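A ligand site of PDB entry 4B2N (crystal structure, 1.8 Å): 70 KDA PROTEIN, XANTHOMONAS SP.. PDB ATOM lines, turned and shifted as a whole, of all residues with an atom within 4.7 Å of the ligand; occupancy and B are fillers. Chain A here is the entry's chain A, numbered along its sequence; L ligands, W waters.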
ATOM      1  N   TRP A 302     -12.216   5.622 -11.260  1.00  0.00           N
ATOM      2  CA  TRP A 302     -13.592   6.130 -11.306  1.00  0.00           C
ATOM      3  C   TRP A 302     -14.238   6.013 -12.652  1.00  0.00           C
ATOM      4  O   TRP A 302     -15.457   5.949 -12.718  1.00  0.00           O
ATOM      5  CB  TRP A 302     -13.627   7.612 -10.895  1.00  0.00           C
ATOM      6  CG  TRP A 302     -13.665   7.704  -9.401  1.00  0.00           C
ATOM      7  CD1 TRP A 302     -12.688   8.172  -8.519  1.00  0.00           C
ATOM      8  CD2 TRP A 302     -14.806   7.361  -8.593  1.00  0.00           C
ATOM      9  NE1 TRP A 302     -13.151   8.133  -7.232  1.00  0.00           N
ATOM     10  CE2 TRP A 302     -14.451   7.674  -7.221  1.00  0.00           C
ATOM     11  CE3 TRP A 302     -16.141   6.913  -8.891  1.00  0.00           C
ATOM     12  CZ2 TRP A 302     -15.328   7.450  -6.175  1.00  0.00           C
ATOM     13  CZ3 TRP A 302     -17.034   6.706  -7.824  1.00  0.00           C
ATOM     14  CH2 TRP A 302     -16.651   6.993  -6.490  1.00  0.00           C
ATOM     15  N   TYR A 367     -34.751  -1.091  -3.805  1.00  0.00           N
ATOM     16  CA  TYR A 367     -33.379  -1.117  -4.402  1.00  0.00           C
ATOM     17  C   TYR A 367     -33.392  -1.921  -5.735  1.00  0.00           C
ATOM     18  O   TYR A 367     -32.922  -1.442  -6.775  1.00  0.00           O
ATOM     19  CB  TYR A 367     -32.373  -1.692  -3.378  1.00  0.00           C
ATOM     20  CG  TYR A 367     -30.970  -1.777  -4.021  1.00  0.00           C
ATOM     21  CD1 TYR A 367     -30.638  -2.817  -4.840  1.00  0.00           C
ATOM     22  CD2 TYR A 367     -30.020  -0.787  -3.808  1.00  0.00           C
ATOM     23  CE1 TYR A 367     -29.412  -2.872  -5.475  1.00  0.00           C
ATOM     24  CE2 TYR A 367     -28.807  -0.838  -4.443  1.00  0.00           C
ATOM     25  CZ  TYR A 367     -28.505  -1.855  -5.265  1.00  0.00           C
ATOM     26  OH  TYR A 367     -27.291  -1.882  -5.895  1.00  0.00           O
ATOM     27  N   LEU A 372     -36.740   3.989 -11.533  1.00  0.00           N
ATOM     28  CA  LEU A 372     -36.655   5.414 -11.235  1.00  0.00           C
ATOM     29  C   LEU A 372     -37.280   6.299 -12.297  1.00  0.00           C
ATOM     30  O   LEU A 372     -37.599   7.465 -12.030  1.00  0.00           O
ATOM     31  CB  LEU A 372     -35.193   5.860 -10.887  1.00  0.00           C
ATOM     32  CG  LEU A 372     -34.677   5.204  -9.589  1.00  0.00           C
ATOM     33  CD1 LEU A 372     -33.192   5.512  -9.433  1.00  0.00           C
ATOM     34  CD2 LEU A 372     -35.439   5.584  -8.332  1.00  0.00           C
ATOM     35  N   TRP A 373     -37.436   5.700 -13.480  1.00  0.00           N
ATOM     36  CA  TRP A 373     -38.097   6.311 -14.628  1.00  0.00           C
ATOM     37  C   TRP A 373     -39.542   5.898 -14.739  1.00  0.00           C
ATOM     38  O   TRP A 373     -40.171   6.197 -15.741  1.00  0.00           O
ATOM     39  CB  TRP A 373     -37.388   5.889 -15.915  1.00  0.00           C
ATOM     40  CG  TRP A 373     -36.045   6.531 -16.111  1.00  0.00           C
ATOM     41  CD1 TRP A 373     -35.734   7.640 -16.916  1.00  0.00           C
ATOM     42  CD2 TRP A 373     -34.773   6.134 -15.476  1.00  0.00           C
ATOM     43  NE1 TRP A 373     -34.396   7.920 -16.846  1.00  0.00           N
ATOM     44  CE2 TRP A 373     -33.759   7.065 -15.985  1.00  0.00           C
ATOM     45  CE3 TRP A 373     -34.387   5.133 -14.584  1.00  0.00           C
ATOM     46  CZ2 TRP A 373     -32.420   6.991 -15.593  1.00  0.00           C
ATOM     47  CZ3 TRP A 373     -33.037   5.067 -14.172  1.00  0.00           C
ATOM     48  CH2 TRP A 373     -32.077   5.973 -14.672  1.00  0.00           C
ATOM     49  N   PRO A 384     -30.493   3.863 -19.088  1.00  0.00           N
ATOM     50  CA  PRO A 384     -29.820   2.684 -19.636  1.00  0.00           C
ATOM     51  C   PRO A 384     -30.688   1.445 -19.757  1.00  0.00           C
ATOM     52  O   PRO A 384     -31.811   1.375 -19.226  1.00  0.00           O
ATOM     53  CB  PRO A 384     -28.688   2.415 -18.644  1.00  0.00           C
ATOM     54  CG  PRO A 384     -28.418   3.739 -17.969  1.00  0.00           C
ATOM     55  CD  PRO A 384     -29.822   4.370 -17.872  1.00  0.00           C
ATOM     56  N   GLY A 388     -34.204   0.168 -14.455  1.00  0.00           N
ATOM     57  CA  GLY A 388     -34.264   1.522 -13.916  1.00  0.00           C
ATOM     58  C   GLY A 388     -34.043   1.604 -12.399  1.00  0.00           C
ATOM     59  O   GLY A 388     -34.233   2.703 -11.781  1.00  0.00           O
ATOM     60  N   SER A 389     -33.711   0.449 -11.800  1.00  0.00           N
ATOM     61  CA  SER A 389     -33.526   0.410 -10.338  1.00  0.00           C
ATOM     62  C   SER A 389     -32.078   0.678  -9.945  1.00  0.00           C
ATOM     63  O   SER A 389     -31.193   0.713 -10.811  1.00  0.00           O
ATOM     64  CB  SER A 389     -33.924  -0.933  -9.790  1.00  0.00           C
ATOM     65  OG  SER A 389     -32.986  -1.919 -10.183  1.00  0.00           O
ATOM     66  N   CYS A 390     -31.833   0.914  -8.649  1.00  0.00           N
ATOM     67  CA  CYS A 390     -30.420   1.027  -8.161  1.00  0.00           C
ATOM     68  C   CYS A 390     -29.588  -0.129  -8.646  1.00  0.00           C
ATOM     69  O   CYS A 390     -28.427   0.024  -9.074  1.00  0.00           O
ATOM     70  CB  CYS A 390     -30.403   0.910  -6.652  1.00  0.00           C
ATOM     71  SG  CYS A 390     -31.540   1.993  -5.775  1.00  0.00           S
ATOM     72  N   SER A 392     -29.890  -1.927 -11.345  1.00  0.00           N
ATOM     73  CA  SER A 392     -29.524  -1.877 -12.756  1.00  0.00           C
ATOM     74  C   SER A 392     -28.187  -1.200 -13.041  1.00  0.00           C
ATOM     75  O   SER A 392     -27.744  -1.211 -14.169  1.00  0.00           O
ATOM     76  CB  SER A 392     -30.617  -1.177 -13.612  1.00  0.00           C
ATOM     77  OG  SER A 392     -30.752   0.194 -13.275  1.00  0.00           O
ATOM     78  N   CYS A 393     -27.580  -0.576 -12.054  1.00  0.00           N
ATOM     79  CA  CYS A 393     -26.247   0.039 -12.259  1.00  0.00           C
ATOM     80  C   CYS A 393     -25.345  -0.494 -11.215  1.00  0.00           C
ATOM     81  O   CYS A 393     -24.284  -1.016 -11.531  1.00  0.00           O
ATOM     82  CB  CYS A 393     -26.264   1.550 -12.084  1.00  0.00           C
ATOM     83  SG  CYS A 393     -27.267   2.268 -13.403  1.00  0.00           S
ATOM     84  N   HIS A 394     -25.750  -0.340  -9.954  1.00  0.00           N
ATOM     85  CA  HIS A 394     -24.836  -0.664  -8.873  1.00  0.00           C
ATOM     86  C   HIS A 394     -24.532  -2.151  -8.685  1.00  0.00           C
ATOM     87  O   HIS A 394     -23.446  -2.554  -8.243  1.00  0.00           O
ATOM     88  CB  HIS A 394     -25.336  -0.045  -7.590  1.00  0.00           C
ATOM     89  CG  HIS A 394     -25.120   1.412  -7.528  1.00  0.00           C
ATOM     90  ND1 HIS A 394     -23.925   1.967  -7.110  1.00  0.00           N
ATOM     91  CD2 HIS A 394     -25.977   2.447  -7.752  1.00  0.00           C
ATOM     92  CE1 HIS A 394     -24.056   3.312  -7.113  1.00  0.00           C
ATOM     93  NE2 HIS A 394     -25.301   3.616  -7.509  1.00  0.00           N
ATOM     94  N   THR A 421     -21.612   4.009 -16.070  1.00  0.00           N
ATOM     95  CA  THR A 421     -22.857   4.668 -16.515  1.00  0.00           C
ATOM     96  C   THR A 421     -22.415   5.820 -17.437  1.00  0.00           C
ATOM     97  O   THR A 421     -21.586   6.659 -17.046  1.00  0.00           O
ATOM     98  CB  THR A 421     -23.656   5.184 -15.307  1.00  0.00           C
ATOM     99  OG1 THR A 421     -23.996   4.114 -14.418  1.00  0.00           O
ATOM    100  CG2 THR A 421     -24.891   5.980 -15.729  1.00  0.00           C
ATOM    101  N   THR A 425     -26.160  10.065 -18.748  1.00  0.00           N
ATOM    102  CA  THR A 425     -27.054   9.633 -17.678  1.00  0.00           C
ATOM    103  C   THR A 425     -26.640   9.962 -16.269  1.00  0.00           C
ATOM    104  O   THR A 425     -27.423  10.542 -15.545  1.00  0.00           O
ATOM    105  CB  THR A 425     -27.783   8.238 -17.880  1.00  0.00           C
ATOM    106  OG1 THR A 425     -27.817   7.448 -16.668  1.00  0.00           O
ATOM    107  CG2 THR A 425     -27.384   7.485 -18.992  1.00  0.00           C
ATOM    108  N   ILE A 426     -25.353   9.717 -15.909  1.00  0.00           N
ATOM    109  CA  ILE A 426     -24.955  10.047 -14.541  1.00  0.00           C
ATOM    110  C   ILE A 426     -24.878  11.541 -14.258  1.00  0.00           C
ATOM    111  O   ILE A 426     -25.321  11.950 -13.186  1.00  0.00           O
ATOM    112  CB  ILE A 426     -23.654   9.313 -14.111  1.00  0.00           C
ATOM    113  CG1 ILE A 426     -23.263   9.656 -12.636  1.00  0.00           C
ATOM    114  CG2 ILE A 426     -22.580   9.416 -15.188  1.00  0.00           C
ATOM    115  CD1 ILE A 426     -24.333   9.048 -11.677  1.00  0.00           C
ATOM    116  N   THR A 428     -22.806  13.580 -13.223  1.00  0.00           N
ATOM    117  CA  THR A 428     -22.045  14.161 -12.110  1.00  0.00           C
ATOM    118  C   THR A 428     -20.912  14.968 -12.706  1.00  0.00           C
ATOM    119  O   THR A 428     -20.704  14.978 -13.943  1.00  0.00           O
ATOM    120  CB  THR A 428     -21.453  13.066 -11.241  1.00  0.00           C
ATOM    121  OG1 THR A 428     -20.977  12.038 -12.108  1.00  0.00           O
ATOM    122  CG2 THR A 428     -22.528  12.490 -10.297  1.00  0.00           C
ATOM    123  N   TYR A 501     -18.829   7.118 -15.498  1.00  0.00           N
ATOM    124  CA  TYR A 501     -18.274   6.755 -14.211  1.00  0.00           C
ATOM    125  C   TYR A 501     -18.825   5.391 -13.770  1.00  0.00           C
ATOM    126  O   TYR A 501     -20.010   5.033 -14.085  1.00  0.00           O
ATOM    127  CB  TYR A 501     -18.581   7.849 -13.162  1.00  0.00           C
ATOM    128  CG  TYR A 501     -18.000   9.182 -13.493  1.00  0.00           C
ATOM    129  CD1 TYR A 501     -16.617   9.363 -13.570  1.00  0.00           C
ATOM    130  CD2 TYR A 501     -18.846  10.310 -13.662  1.00  0.00           C
ATOM    131  CE1 TYR A 501     -16.090  10.628 -13.886  1.00  0.00           C
ATOM    132  CE2 TYR A 501     -18.345  11.559 -13.957  1.00  0.00           C
ATOM    133  CZ  TYR A 501     -16.950  11.712 -14.064  1.00  0.00           C
ATOM    134  OH  TYR A 501     -16.453  12.951 -14.367  1.00  0.00           O
ATOM    135  N   ILE A 502     -17.999   4.621 -13.057  1.00  0.00           N
ATOM    136  CA  ILE A 502     -18.425   3.348 -12.478  1.00  0.00           C
ATOM    137  C   ILE A 502     -19.530   3.635 -11.408  1.00  0.00           C
ATOM    138  O   ILE A 502     -19.440   4.647 -10.679  1.00  0.00           O
ATOM    139  CB  ILE A 502     -17.198   2.643 -11.858  1.00  0.00           C
ATOM    140  CG1 ILE A 502     -17.536   1.243 -11.374  1.00  0.00           C
ATOM    141  CG2 ILE A 502     -16.684   3.436 -10.674  1.00  0.00           C
ATOM    142  CD1 ILE A 502     -17.904   0.326 -12.527  1.00  0.00           C
ATOM    143  N   ALA A 503     -20.629   2.845 -11.400  1.00  0.00           N
ATOM    144  CA  ALA A 503     -21.575   2.826 -10.262  1.00  0.00           C
ATOM    145  C   ALA A 503     -20.915   1.911  -9.178  1.00  0.00           C
ATOM    146  O   ALA A 503     -20.843   0.668  -9.302  1.00  0.00           O
ATOM    147  CB  ALA A 503     -22.975   2.354 -10.702  1.00  0.00           C
ATOM    148  N   PRO A 504     -20.338   2.508  -8.130  1.00  0.00           N
ATOM    149  CA  PRO A 504     -19.495   1.602  -7.298  1.00  0.00           C
ATOM    150  C   PRO A 504     -20.330   0.700  -6.371  1.00  0.00           C
ATOM    151  O   PRO A 504     -21.499   0.963  -6.198  1.00  0.00           O
ATOM    152  CB  PRO A 504     -18.695   2.558  -6.410  1.00  0.00           C
ATOM    153  CG  PRO A 504     -19.491   3.837  -6.400  1.00  0.00           C
ATOM    154  CD  PRO A 504     -20.242   3.915  -7.719  1.00  0.00           C
ATOM    155  N   LEU A 506     -22.089  -0.644  -3.149  1.00  0.00           N
ATOM    156  CA  LEU A 506     -22.667  -0.008  -1.958  1.00  0.00           C
ATOM    157  C   LEU A 506     -22.430  -0.775  -0.674  1.00  0.00           C
ATOM    158  O   LEU A 506     -22.774  -0.273   0.387  1.00  0.00           O
ATOM    159  CB  LEU A 506     -24.146   0.361  -2.124  1.00  0.00           C
ATOM    160  CG  LEU A 506     -24.483   1.120  -3.410  1.00  0.00           C
ATOM    161  CD1 LEU A 506     -25.956   1.454  -3.462  1.00  0.00           C
ATOM    162  CD2 LEU A 506     -23.744   2.454  -3.410  1.00  0.00           C
ATOM    163  N   TYR A 515     -19.960  11.489  -0.705  1.00  0.00           N
ATOM    164  CA  TYR A 515     -20.179  10.612  -1.836  1.00  0.00           C
ATOM    165  C   TYR A 515     -19.863  11.259  -3.224  1.00  0.00           C
ATOM    166  O   TYR A 515     -19.769  12.505  -3.336  1.00  0.00           O
ATOM    167  CB  TYR A 515     -21.649  10.114  -1.802  1.00  0.00           C
ATOM    168  CG  TYR A 515     -21.902   9.355  -0.516  1.00  0.00           C
ATOM    169  CD1 TYR A 515     -21.334   8.090  -0.316  1.00  0.00           C
ATOM    170  CD2 TYR A 515     -22.643   9.921   0.530  1.00  0.00           C
ATOM    171  CE1 TYR A 515     -21.541   7.408   0.885  1.00  0.00           C
ATOM    172  CE2 TYR A 515     -22.876   9.248   1.732  1.00  0.00           C
ATOM    173  CZ  TYR A 515     -22.302   7.963   1.882  1.00  0.00           C
ATOM    174  OH  TYR A 515     -22.420   7.240   3.023  1.00  0.00           O
ATOM    175  N   PHE A 516     -19.857  10.421  -4.269  1.00  0.00           N
ATOM    176  CA  PHE A 516     -19.480  10.741  -5.613  1.00  0.00           C
ATOM    177  C   PHE A 516     -17.976  10.863  -5.731  1.00  0.00           C
ATOM    178  O   PHE A 516     -17.275  11.016  -4.732  1.00  0.00           O
ATOM    179  CB  PHE A 516     -20.184  11.987  -6.203  1.00  0.00           C
ATOM    180  CG  PHE A 516     -21.678  11.863  -6.232  1.00  0.00           C
ATOM    181  CD1 PHE A 516     -22.269  10.613  -6.242  1.00  0.00           C
ATOM    182  CD2 PHE A 516     -22.469  13.007  -6.279  1.00  0.00           C
ATOM    183  CE1 PHE A 516     -23.672  10.471  -6.278  1.00  0.00           C
ATOM    184  CE2 PHE A 516     -23.863  12.911  -6.319  1.00  0.00           C
ATOM    185  CZ  PHE A 516     -24.449  11.635  -6.321  1.00  0.00           C
ATOM    186  N   HIS A 517     -17.512  10.835  -6.966  1.00  0.00           N
ATOM    187  CA  HIS A 517     -16.063  10.746  -7.230  1.00  0.00           C
ATOM    188  C   HIS A 517     -15.310  11.945  -6.727  1.00  0.00           C
ATOM    189  O   HIS A 517     -14.116  11.864  -6.618  1.00  0.00           O
ATOM    190  CB  HIS A 517     -15.820  10.504  -8.699  1.00  0.00           C
ATOM    191  CG  HIS A 517     -16.204  11.663  -9.567  1.00  0.00           C
ATOM    192  ND1 HIS A 517     -17.508  11.849 -10.071  1.00  0.00           N
ATOM    193  CD2 HIS A 517     -15.445  12.699 -10.056  1.00  0.00           C
ATOM    194  CE1 HIS A 517     -17.498  12.969 -10.833  1.00  0.00           C
ATOM    195  NE2 HIS A 517     -16.252  13.488 -10.826  1.00  0.00           N
ATOM    196  N   LEU A 524     -26.072  10.251   2.441  1.00  0.00           N
ATOM    197  CA  LEU A 524     -26.740   9.403   1.483  1.00  0.00           C
ATOM    198  C   LEU A 524     -28.098   9.947   1.094  1.00  0.00           C
ATOM    199  O   LEU A 524     -28.531   9.871  -0.116  1.00  0.00           O
ATOM    200  CB  LEU A 524     -26.856   7.987   2.052  1.00  0.00           C
ATOM    201  CG  LEU A 524     -26.416   7.024   0.963  1.00  0.00           C
ATOM    202  CD1 LEU A 524     -25.539   5.958   1.541  1.00  0.00           C
ATOM    203  CD2 LEU A 524     -27.659   6.466   0.248  1.00  0.00           C
ATOM    204  N   VAL A 527     -27.616  12.109  -1.924  1.00  0.00           N
ATOM    205  CA  VAL A 527     -27.552  11.326  -3.140  1.00  0.00           C
ATOM    206  C   VAL A 527     -28.989  11.006  -3.568  1.00  0.00           C
ATOM    207  O   VAL A 527     -29.304  11.079  -4.749  1.00  0.00           O
ATOM    208  CB  VAL A 527     -26.757  10.042  -2.868  1.00  0.00           C
ATOM    209  CG1 VAL A 527     -26.792   9.122  -4.090  1.00  0.00           C
ATOM    210  CG2 VAL A 527     -25.311  10.414  -2.476  1.00  0.00           C
ATOM    211  N   LEU A 528     -29.809  10.667  -2.579  1.00  0.00           N
ATOM    212  CA  LEU A 528     -31.191  10.210  -2.844  1.00  0.00           C
ATOM    213  C   LEU A 528     -32.157  11.344  -3.108  1.00  0.00           C
ATOM    214  O   LEU A 528     -33.247  11.153  -3.658  1.00  0.00           O
ATOM    215  CB  LEU A 528     -31.652   9.293  -1.712  1.00  0.00           C
ATOM    216  CG  LEU A 528     -30.932   7.924  -1.739  1.00  0.00           C
ATOM    217  CD1 LEU A 528     -31.512   7.055  -0.661  1.00  0.00           C
ATOM    218  CD2 LEU A 528     -31.010   7.192  -3.061  1.00  0.00           C
ATOM    219  N   HIS A 641     -26.606  12.344 -10.802  1.00  0.00           N
ATOM    220  CA  HIS A 641     -27.278  11.245 -10.177  1.00  0.00           C
ATOM    221  C   HIS A 641     -28.672  11.745  -9.725  1.00  0.00           C
ATOM    222  O   HIS A 641     -29.152  11.409  -8.649  1.00  0.00           O
ATOM    223  CB  HIS A 641     -26.420  10.791  -8.976  1.00  0.00           C
ATOM    224  CG  HIS A 641     -26.768   9.425  -8.470  1.00  0.00           C
ATOM    225  ND1 HIS A 641     -27.819   9.191  -7.666  1.00  0.00           N
ATOM    226  CD2 HIS A 641     -26.110   8.214  -8.634  1.00  0.00           C
ATOM    227  CE1 HIS A 641     -27.814   7.884  -7.317  1.00  0.00           C
ATOM    228  NE2 HIS A 641     -26.775   7.300  -7.915  1.00  0.00           N
ATOM    229  N   PHE A 643     -31.639  11.270 -11.130  1.00  0.00           N
ATOM    230  CA  PHE A 643     -32.781  10.351 -11.308  1.00  0.00           C
ATOM    231  C   PHE A 643     -33.375   9.879  -9.980  1.00  0.00           C
ATOM    232  O   PHE A 643     -34.464   9.379  -9.941  1.00  0.00           O
ATOM    233  CB  PHE A 643     -32.398   9.154 -12.140  1.00  0.00           C
ATOM    234  CG  PHE A 643     -30.972   8.692 -11.890  1.00  0.00           C
ATOM    235  CD1 PHE A 643     -30.632   7.971 -10.738  1.00  0.00           C
ATOM    236  CD2 PHE A 643     -30.009   8.983 -12.822  1.00  0.00           C
ATOM    237  CE1 PHE A 643     -29.290   7.569 -10.501  1.00  0.00           C
ATOM    238  CE2 PHE A 643     -28.618   8.637 -12.584  1.00  0.00           C
ATOM    239  CZ  PHE A 643     -28.302   7.894 -11.465  1.00  0.00           C
ATOM    240  N   THR A 644     -32.645  10.021  -8.884  1.00  0.00           N
ATOM    241  CA  THR A 644     -33.232   9.748  -7.576  1.00  0.00           C
ATOM    242  C   THR A 644     -34.363  10.731  -7.113  1.00  0.00           C
ATOM    243  O   THR A 644     -35.077  10.465  -6.137  1.00  0.00           O
ATOM    244  CB  THR A 644     -32.149   9.683  -6.537  1.00  0.00           C
ATOM    245  OG1 THR A 644     -31.434  10.922  -6.535  1.00  0.00           O
ATOM    246  CG2 THR A 644     -31.175   8.581  -6.893  1.00  0.00           C
ATOM    247  N   LEU A 647     -37.951   9.520  -6.477  1.00  0.00           N
ATOM    248  CA  LEU A 647     -38.270   8.748  -5.263  1.00  0.00           C
ATOM    249  C   LEU A 647     -39.192   9.518  -4.336  1.00  0.00           C
ATOM    250  O   LEU A 647     -39.269  10.742  -4.412  1.00  0.00           O
ATOM    251  CB  LEU A 647     -37.003   8.387  -4.468  1.00  0.00           C
ATOM    252  CG  LEU A 647     -36.122   7.464  -5.263  1.00  0.00           C
ATOM    253  CD1 LEU A 647     -34.743   7.488  -4.609  1.00  0.00           C
ATOM    254  CD2 LEU A 647     -36.696   6.041  -5.179  1.00  0.00           C
ATOM    255  N   LEU A 655     -34.697   2.908   1.573  1.00  0.00           N
ATOM    256  CA  LEU A 655     -33.459   2.631   0.859  1.00  0.00           C
ATOM    257  C   LEU A 655     -32.275   2.894   1.777  1.00  0.00           C
ATOM    258  O   LEU A 655     -31.307   2.118   1.759  1.00  0.00           O
ATOM    259  CB  LEU A 655     -33.353   3.524  -0.364  1.00  0.00           C
ATOM    260  CG  LEU A 655     -34.068   3.113  -1.658  1.00  0.00           C
ATOM    261  CD1 LEU A 655     -34.046   4.347  -2.560  1.00  0.00           C
ATOM    262  CD2 LEU A 655     -33.401   1.907  -2.349  1.00  0.00           C
ATOM    263  N   ILE A 659     -29.410   0.197   2.970  1.00  0.00           N
ATOM    264  CA  ILE A 659     -27.956   0.381   2.737  1.00  0.00           C
ATOM    265  C   ILE A 659     -27.154   0.104   4.025  1.00  0.00           C
ATOM    266  O   ILE A 659     -25.961  -0.316   3.995  1.00  0.00           O
ATOM    267  CB  ILE A 659     -27.643   1.743   2.109  1.00  0.00           C
ATOM    268  CG1 ILE A 659     -28.179   1.780   0.659  1.00  0.00           C
ATOM    269  CG2 ILE A 659     -26.108   2.029   2.150  1.00  0.00           C
ATOM    270  CD1 ILE A 659     -28.444   3.149   0.124  1.00  0.00           C
HETATM  271 FE1  LIG L   1     -26.071   5.459  -7.818  1.00  0.00          FE
HETATM  272  C1  LIG L   1     -23.052   6.946  -7.056  1.00  0.00           C
HETATM  273  C2  LIG L   1     -26.753   4.884  -4.362  1.00  0.00           C
HETATM  274  C3  LIG L   1     -29.262   4.444  -8.496  1.00  0.00           C
HETATM  275  C4  LIG L   1     -25.058   4.971 -11.044  1.00  0.00           C
HETATM  276  N1  LIG L   1     -25.053   5.735  -6.096  1.00  0.00           N
HETATM  277  C5  LIG L   1     -23.870   6.518  -5.954  1.00  0.00           C
HETATM  278  C6  LIG L   1     -23.515   6.697  -4.552  1.00  0.00           C
HETATM  279  C7  LIG L   1     -24.599   6.084  -3.761  1.00  0.00           C
HETATM  280  C8  LIG L   1     -25.541   5.574  -4.738  1.00  0.00           C
HETATM  281  C9  LIG L   1     -24.661   5.995  -2.250  1.00  0.00           C
HETATM  282  C10 LIG L   1     -22.234   7.292  -3.976  1.00  0.00           C
HETATM  283  C11 LIG L   1     -21.260   6.057  -4.053  1.00  0.00           C
HETATM  284  C12 LIG L   1     -19.819   6.487  -3.746  1.00  0.00           C
HETATM  285  O1  LIG L   1     -19.604   7.718  -3.631  1.00  0.00           O
HETATM  286  O2  LIG L   1     -18.847   5.663  -3.560  1.00  0.00           O
HETATM  287  N2  LIG L   1     -27.721   4.795  -6.587  1.00  0.00           N
HETATM  288  C13 LIG L   1     -27.853   4.604  -5.273  1.00  0.00           C
HETATM  289  C14 LIG L   1     -29.155   4.127  -4.817  1.00  0.00           C
HETATM  290  C15 LIG L   1     -29.924   4.014  -6.074  1.00  0.00           C
HETATM  291  C16 LIG L   1     -28.945   4.446  -7.077  1.00  0.00           C
HETATM  292  C17 LIG L   1     -29.562   3.822  -3.395  1.00  0.00           C
HETATM  293  C18 LIG L   1     -31.360   3.612  -6.288  1.00  0.00           C
HETATM  294  C19 LIG L   1     -32.289   4.525  -5.757  1.00  0.00           C
HETATM  295  N3  LIG L   1     -26.946   4.710  -9.382  1.00  0.00           N
HETATM  296  C20 LIG L   1     -28.332   4.480  -9.588  1.00  0.00           C
HETATM  297  C21 LIG L   1     -28.732   4.231 -10.962  1.00  0.00           C
HETATM  298  C22 LIG L   1     -27.493   4.374 -11.703  1.00  0.00           C
HETATM  299  C23 LIG L   1     -26.443   4.762 -10.714  1.00  0.00           C
HETATM  300  C24 LIG L   1     -30.109   3.899 -11.510  1.00  0.00           C
HETATM  301  C25 LIG L   1     -27.382   4.233 -13.191  1.00  0.00           C
HETATM  302  C26 LIG L   1     -28.145   4.875 -14.092  1.00  0.00           C
HETATM  303  N4  LIG L   1     -24.391   5.798  -8.812  1.00  0.00           N
HETATM  304  C27 LIG L   1     -24.132   5.633 -10.099  1.00  0.00           C
HETATM  305  C28 LIG L   1     -22.830   6.075 -10.605  1.00  0.00           C
HETATM  306  C29 LIG L   1     -22.241   6.671  -9.431  1.00  0.00           C
HETATM  307  C30 LIG L   1     -23.265   6.480  -8.418  1.00  0.00           C
HETATM  308  C31 LIG L   1     -22.274   5.956 -11.996  1.00  0.00           C
HETATM  309  C32 LIG L   1     -20.869   7.311  -9.338  1.00  0.00           C
HETATM  310  C33 LIG L   1     -21.127   8.824  -9.497  1.00  0.00           C
HETATM  311  C34 LIG L   1     -19.873   9.638  -9.381  1.00  0.00           C
HETATM  312  O3  LIG L   1     -19.526  10.443 -10.255  1.00  0.00           O
HETATM  313  O4  LIG L   1     -19.210   9.419  -8.390  1.00  0.00           O
HETATM  314  O   HOH W   1     -18.120   6.711  -0.826  1.00  0.00           O
HETATM  315  O   HOH W   2     -16.675   4.469  -4.335  1.00  0.00           O
HETATM  316  O   HOH W   3     -20.150   3.257  -2.361  1.00  0.00           O
HETATM  317  O   HOH W   4     -16.059   4.619  -1.820  1.00  0.00           O
HETATM  318  O   HOH W   5     -16.946   8.375  -3.204  1.00  0.00           O
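N of Ile 502 sits at hydrogen-bond distance from O of Trp 302.
N of His 641 lies within hydrogen-bond range of O of Ile 426.
O of Tyr 367 sits at hydrogen-bond distance from N of Cys 390, 3.2 Å away.
O of Val 527 sits at hydrogen-bond distance from OG1 of Thr 644 (2.8 Å).
The backbone carbonyl oxygen (O) of Ser 389 lies within hydrogen-bond range of the side-chain hydroxyl (OG) of Ser 392, at 2.6 Å.
The backbone carbonyl oxygen (O) of His 641 lies within hydrogen-bond range of the side-chain hydroxyl (OG1) of Thr 644, 3.1 Å away.
The backbone carbonyl oxygen (O) of Leu 528 lies within hydrogen-bond range of the side-chain hydroxyl (OG1) of Thr 644 (3.4 Å).
ND1 of His 394 lies within hydrogen-bond range of O of Pro 504 (2.8 Å).
Trp 302 touches the ligand.
Leu 372 touches the ligand (CD1 to C19, 3.9 Å).
Ser 389 touches the ligand.
OG1 of Thr 421 touches C31 of the ligand, at 3.5 Å.
Thr 425 touches the ligand.
Ile 426 touches the ligand.
O of Tyr 501 touches C31 of the ligand, at 3.2 Å.
O of Ile 502 touches C32 of the ligand, 3.3 Å away.
Ala 503 touches the ligand.
Pro 504 touches the ligand.
Leu 506 touches the ligand (CD1 to C2, 3.6 Å).
CA of Tyr 515 touches O1 of the ligand, at 3.5 Å.
Leu 524 touches the ligand.
CG1 of Val 527 touches C7 of the ligand, at 3.8 Å.
CD2 of Leu 528 touches C17 of the ligand, at 3.7 Å.
Phe 643 touches the ligand.
Leu 655 touches the ligand (CD1 to C19, 3.7 Å).
Ile 659 touches the ligand (CD1 to C17, 3.8 Å).
Hydrophobic or aromatic side chains that line the ligand: Trp 302, Leu 372, His 394, Ile 426, Tyr 501, Ala 503, Pro 504, Leu 506, Tyr 515, Phe 516, His 517, Leu 524, Val 527, Leu 528, His 641, Phe 643, Leu 655 and Ile 659.
The nearest printed residue that does not touch the ligand is Leu 647 (4.01 Å).
Water W5 lies within hydrogen-bond range of O1 of the ligand (2.8 Å) and O of Phe 516 (3.1 Å).
An oxygen (O3) of the ligand lies within hydrogen-bond range of the side-chain hydroxyl (OG1) of Thr 428 (2.8 Å).
An iron atom (FE1) of the ligand is bound by a ring nitrogen (NE2) of His 641 (2.0 Å).
FE1 of the ligand is bound by NE2 of His 394.
The side-chain sulfur of Cys 393 is covalently linked to a carbon (C25) of the ligand, 2.0 Å away.
The backbone NH (N) of His 517 sits at hydrogen-bond distance from an oxygen (O4) of the ligand (2.6 Å).
O3 of the ligand is in hydrogen-bond range of ND1 of His 517 (2.5 Å).
N of Phe 516 sits at hydrogen-bond distance from O1 of the ligand, 2.8 Å away.
The side-chain sulfur (SG) of Cys 390 is bonded to a carbon (C18) of the ligand (1.7 Å).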
